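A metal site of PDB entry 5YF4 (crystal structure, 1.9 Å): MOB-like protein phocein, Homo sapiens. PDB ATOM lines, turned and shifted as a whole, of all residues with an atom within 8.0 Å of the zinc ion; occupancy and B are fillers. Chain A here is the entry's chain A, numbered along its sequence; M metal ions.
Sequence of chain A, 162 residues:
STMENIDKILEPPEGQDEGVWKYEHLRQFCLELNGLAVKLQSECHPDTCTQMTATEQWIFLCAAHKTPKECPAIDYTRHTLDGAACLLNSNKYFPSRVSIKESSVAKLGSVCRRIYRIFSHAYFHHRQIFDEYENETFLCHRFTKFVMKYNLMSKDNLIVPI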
ATOM      1  N   LEU A  61      12.712  24.060 -16.593  1.00  0.00           N
ATOM      2  CA  LEU A  61      13.105  22.679 -16.328  1.00  0.00           C
ATOM      3  C   LEU A  61      14.127  22.242 -17.364  1.00  0.00           C
ATOM      4  O   LEU A  61      13.905  22.408 -18.575  1.00  0.00           O
ATOM      5  CB  LEU A  61      11.904  21.745 -16.350  1.00  0.00           C
ATOM      6  CG  LEU A  61      10.770  22.083 -15.379  1.00  0.00           C
ATOM      7  CD1 LEU A  61       9.736  20.936 -15.365  1.00  0.00           C
ATOM      8  CD2 LEU A  61      11.280  22.366 -13.987  1.00  0.00           C
ATOM      9  N   CYS A  62      15.253  21.711 -16.877  1.00  0.00           N
ATOM     10  CA  CYS A  62      16.360  21.281 -17.724  1.00  0.00           C
ATOM     11  C   CYS A  62      15.965  20.114 -18.605  1.00  0.00           C
ATOM     12  O   CYS A  62      15.434  19.125 -18.113  1.00  0.00           O
ATOM     13  CB  CYS A  62      17.544  20.882 -16.845  1.00  0.00           C
ATOM     14  SG  CYS A  62      19.014  20.479 -17.771  1.00  0.00           S
ATOM     15  N   ALA A  63      16.222  20.217 -19.921  1.00  0.00           N
ATOM     16  CA  ALA A  63      15.776  19.223 -20.891  1.00  0.00           C
ATOM     17  C   ALA A  63      16.815  18.108 -21.128  1.00  0.00           C
ATOM     18  O   ALA A  63      16.551  17.215 -21.945  1.00  0.00           O
ATOM     19  CB  ALA A  63      15.412  19.895 -22.221  1.00  0.00           C
ATOM     20  N   ALA A  64      17.970  18.113 -20.445  1.00  0.00           N
ATOM     21  CA  ALA A  64      19.008  17.111 -20.691  1.00  0.00           C
ATOM     22  C   ALA A  64      18.787  15.838 -19.900  1.00  0.00           C
ATOM     23  O   ALA A  64      19.748  15.187 -19.490  1.00  0.00           O
ATOM     24  CB  ALA A  64      20.401  17.678 -20.374  1.00  0.00           C
ATOM     25  N   HIS A  65      17.531  15.457 -19.716  1.00  0.00           N
ATOM     26  CA  HIS A  65      17.177  14.337 -18.865  1.00  0.00           C
ATOM     27  C   HIS A  65      15.971  13.659 -19.498  1.00  0.00           C
ATOM     28  O   HIS A  65      15.328  14.232 -20.381  1.00  0.00           O
ATOM     29  CB  HIS A  65      16.858  14.854 -17.468  1.00  0.00           C
ATOM     30  CG  HIS A  65      17.972  15.674 -16.861  1.00  0.00           C
ATOM     31  ND1 HIS A  65      19.045  15.112 -16.223  1.00  0.00           N
ATOM     32  CD2 HIS A  65      18.168  17.020 -16.824  1.00  0.00           C
ATOM     33  CE1 HIS A  65      19.867  16.068 -15.797  1.00  0.00           C
ATOM     34  NE2 HIS A  65      19.358  17.230 -16.153  1.00  0.00           N
ATOM     35  N   THR A  67      13.073  13.005 -18.300  1.00  0.00           N
ATOM     36  CA  THR A  67      11.984  13.898 -17.945  1.00  0.00           C
ATOM     37  C   THR A  67      12.543  15.253 -17.529  1.00  0.00           C
ATOM     38  O   THR A  67      13.549  15.302 -16.832  1.00  0.00           O
ATOM     39  CB  THR A  67      11.183  13.280 -16.804  1.00  0.00           C
ATOM     40  OG1 THR A  67      10.603  12.060 -17.275  1.00  0.00           O
ATOM     41  CG2 THR A  67      10.094  14.194 -16.337  1.00  0.00           C
ATOM     42  N   PRO A  68      11.932  16.364 -17.956  1.00  0.00           N
ATOM     43  CA  PRO A  68      12.462  17.696 -17.592  1.00  0.00           C
ATOM     44  C   PRO A  68      12.624  17.793 -16.071  1.00  0.00           C
ATOM     45  O   PRO A  68      11.736  17.418 -15.321  1.00  0.00           O
ATOM     46  CB  PRO A  68      11.381  18.661 -18.111  1.00  0.00           C
ATOM     47  CG  PRO A  68      10.788  17.893 -19.303  1.00  0.00           C
ATOM     48  CD  PRO A  68      10.767  16.447 -18.868  1.00  0.00           C
ATOM     49  N   LYS A  69      13.776  18.301 -15.635  1.00  0.00           N
ATOM     50  CA  LYS A  69      14.253  18.229 -14.257  1.00  0.00           C
ATOM     51  C   LYS A  69      14.470  19.635 -13.716  1.00  0.00           C
ATOM     52  O   LYS A  69      14.888  20.538 -14.450  1.00  0.00           O
ATOM     53  CB  LYS A  69      15.556  17.446 -14.217  1.00  0.00           C
ATOM     54  CG  LYS A  69      16.221  17.257 -12.847  1.00  0.00           C
ATOM     55  CD  LYS A  69      17.481  16.366 -13.073  1.00  0.00           C
ATOM     56  CE  LYS A  69      18.352  16.179 -11.771  1.00  0.00           C
ATOM     57  NZ  LYS A  69      19.028  17.457 -11.385  1.00  0.00           N
ATOM     58  N   GLU A  70      14.175  19.820 -12.427  1.00  0.00           N
ATOM     59  CA  GLU A  70      14.394  21.085 -11.737  1.00  0.00           C
ATOM     60  C   GLU A  70      15.873  21.219 -11.335  1.00  0.00           C
ATOM     61  O   GLU A  70      16.229  21.171 -10.158  1.00  0.00           O
ATOM     62  CB  GLU A  70      13.536  21.163 -10.496  1.00  0.00           C
ATOM     63  CG  GLU A  70      12.191  21.826 -10.625  1.00  0.00           C
ATOM     64  CD  GLU A  70      11.573  22.086  -9.238  1.00  0.00           C
ATOM     65  OE1 GLU A  70      11.921  23.118  -8.598  1.00  0.00           O
ATOM     66  OE2 GLU A  70      10.793  21.211  -8.790  1.00  0.00           O
ATOM     67  N   CYS A  71      16.723  21.350 -12.324  1.00  0.00           N
ATOM     68  CA  CYS A  71      18.144  21.491 -12.024  1.00  0.00           C
ATOM     69  C   CYS A  71      18.412  22.871 -11.412  1.00  0.00           C
ATOM     70  O   CYS A  71      17.794  23.853 -11.818  1.00  0.00           O
ATOM     71  CB  CYS A  71      18.974  21.332 -13.305  1.00  0.00           C
ATOM     72  SG  CYS A  71      18.990  19.573 -13.905  1.00  0.00           S
ATOM     73  N   PRO A  72      19.345  22.958 -10.459  1.00  0.00           N
ATOM     74  CA  PRO A  72      19.837  24.272 -10.036  1.00  0.00           C
ATOM     75  C   PRO A  72      20.399  24.999 -11.231  1.00  0.00           C
ATOM     76  O   PRO A  72      20.801  24.393 -12.240  1.00  0.00           O
ATOM     77  CB  PRO A  72      20.960  23.933  -9.034  1.00  0.00           C
ATOM     78  CG  PRO A  72      20.785  22.498  -8.706  1.00  0.00           C
ATOM     79  CD  PRO A  72      20.124  21.854  -9.886  1.00  0.00           C
ATOM     80  N   ILE A  74      23.107  26.439 -12.078  1.00  0.00           N
ATOM     81  CA  ILE A  74      24.415  26.091 -12.585  1.00  0.00           C
ATOM     82  C   ILE A  74      24.373  24.803 -13.395  1.00  0.00           C
ATOM     83  O   ILE A  74      25.032  24.681 -14.345  1.00  0.00           O
ATOM     84  CB  ILE A  74      25.491  26.118 -11.474  1.00  0.00           C
ATOM     85  CG1 ILE A  74      26.860  26.417 -12.049  1.00  0.00           C
ATOM     86  CG2 ILE A  74      25.411  24.954 -10.547  1.00  0.00           C
ATOM     87  CD1 ILE A  74      27.744  25.220 -12.207  1.00  0.00           C
ATOM     88  N   ASP A  75      23.580  23.870 -12.906  1.00  0.00           N
ATOM     89  CA  ASP A  75      23.372  22.615 -13.624  1.00  0.00           C
ATOM     90  C   ASP A  75      22.605  22.847 -14.928  1.00  0.00           C
ATOM     91  O   ASP A  75      22.943  22.264 -15.963  1.00  0.00           O
ATOM     92  CB  ASP A  75      22.577  21.648 -12.759  1.00  0.00           C
ATOM     93  CG  ASP A  75      23.432  20.964 -11.705  1.00  0.00           C
ATOM     94  OD1 ASP A  75      22.918  20.052 -11.014  1.00  0.00           O
ATOM     95  OD2 ASP A  75      24.621  21.318 -11.578  1.00  0.00           O
ATOM     96  N   TYR A  76      21.496  23.578 -14.850  1.00  0.00           N
ATOM     97  CA  TYR A  76      20.740  23.896 -16.068  1.00  0.00           C
ATOM     98  C   TYR A  76      21.678  24.465 -17.121  1.00  0.00           C
ATOM     99  O   TYR A  76      21.662  24.059 -18.296  1.00  0.00           O
ATOM    100  CB  TYR A  76      19.656  24.934 -15.768  1.00  0.00           C
ATOM    101  CG  TYR A  76      18.809  25.231 -17.017  1.00  0.00           C
ATOM    102  CD1 TYR A  76      19.276  26.098 -18.014  1.00  0.00           C
ATOM    103  CD2 TYR A  76      17.528  24.696 -17.152  1.00  0.00           C
ATOM    104  CE1 TYR A  76      18.534  26.349 -19.144  1.00  0.00           C
ATOM    105  CE2 TYR A  76      16.741  24.981 -18.330  1.00  0.00           C
ATOM    106  CZ  TYR A  76      17.267  25.799 -19.290  1.00  0.00           C
ATOM    107  OH  TYR A  76      16.525  26.088 -20.442  1.00  0.00           O
ATOM    108  N   THR A  77      22.512  25.429 -16.709  1.00  0.00           N
ATOM    109  CA  THR A  77      23.448  26.081 -17.633  1.00  0.00           C
ATOM    110  C   THR A  77      24.381  25.075 -18.295  1.00  0.00           C
ATOM    111  O   THR A  77      24.490  25.021 -19.523  1.00  0.00           O
ATOM    112  CB  THR A  77      24.218  27.156 -16.872  1.00  0.00           C
ATOM    113  OG1 THR A  77      23.257  28.147 -16.469  1.00  0.00           O
ATOM    114  CG2 THR A  77      25.259  27.834 -17.765  1.00  0.00           C
ATOM    115  N   ARG A  78      25.056  24.264 -17.477  1.00  0.00           N
ATOM    116  CA  ARG A  78      26.031  23.289 -17.987  1.00  0.00           C
ATOM    117  C   ARG A  78      25.367  22.250 -18.866  1.00  0.00           C
ATOM    118  O   ARG A  78      25.879  21.905 -19.948  1.00  0.00           O
ATOM    119  CB  ARG A  78      26.739  22.614 -16.796  1.00  0.00           C
ATOM    120  CG  ARG A  78      27.839  21.603 -17.193  1.00  0.00           C
ATOM    121  CD  ARG A  78      29.104  22.365 -17.710  1.00  0.00           C
ATOM    122  NE  ARG A  78      29.131  22.533 -19.167  1.00  0.00           N
ATOM    123  CZ  ARG A  78      29.518  23.656 -19.804  1.00  0.00           C
ATOM    124  NH1 ARG A  78      29.910  24.730 -19.118  1.00  0.00           N
ATOM    125  NH2 ARG A  78      29.520  23.687 -21.131  1.00  0.00           N
ATOM    126  N   HIS A  79      24.275  21.656 -18.379  1.00  0.00           N
ATOM    127  CA  HIS A  79      23.647  20.557 -19.106  1.00  0.00           C
ATOM    128  C   HIS A  79      23.104  21.056 -20.442  1.00  0.00           C
ATOM    129  O   HIS A  79      23.163  20.337 -21.446  1.00  0.00           O
ATOM    130  CB  HIS A  79      22.489  19.953 -18.284  1.00  0.00           C
ATOM    131  CG  HIS A  79      22.887  19.416 -16.949  1.00  0.00           C
ATOM    132  ND1 HIS A  79      21.955  19.098 -15.976  1.00  0.00           N
ATOM    133  CD2 HIS A  79      24.102  19.092 -16.427  1.00  0.00           C
ATOM    134  CE1 HIS A  79      22.573  18.629 -14.901  1.00  0.00           C
ATOM    135  NE2 HIS A  79      23.879  18.604 -15.158  1.00  0.00           N
ATOM    136  N   THR A  80      22.574  22.282 -20.455  1.00  0.00           N
ATOM    137  CA  THR A  80      21.998  22.844 -21.684  1.00  0.00           C
ATOM    138  C   THR A  80      23.096  23.186 -22.703  1.00  0.00           C
ATOM    139  O   THR A  80      22.955  22.873 -23.887  1.00  0.00           O
ATOM    140  CB  THR A  80      21.156  24.076 -21.344  1.00  0.00           C
ATOM    141  OG1 THR A  80      20.081  23.676 -20.481  1.00  0.00           O
ATOM    142  CG2 THR A  80      20.618  24.729 -22.618  1.00  0.00           C
HETATM  143 ZN    ZN M   1      19.903  19.222 -16.017  1.00  0.00          ZN
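A ring nitrogen (ND1) of His 79 sits close to the backbone carbonyl oxygen (O) of Asp 75, at 3.3 Å. SG of Cys 71 lies close to NZ of Lys 69. The side-chain sulfur (SG) of Cys 62 lies close to the backbone NH (N) of Ala 64, at 3.7 Å. The backbone carbonyl oxygen (O) of Lys 69 lies within hydrogen-bond range of the backbone NH (N) of Cys 62 (2.7 Å).
Within 4 Å of the zinc ion: Cys 62, His 65, Cys 71 and His 79.
The zinc ion is bound by ND1 of His 79, NE2 of His 65, SG of Cys 71 and SG of Cys 62. The zinc ion has four donor atoms within binding distance.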
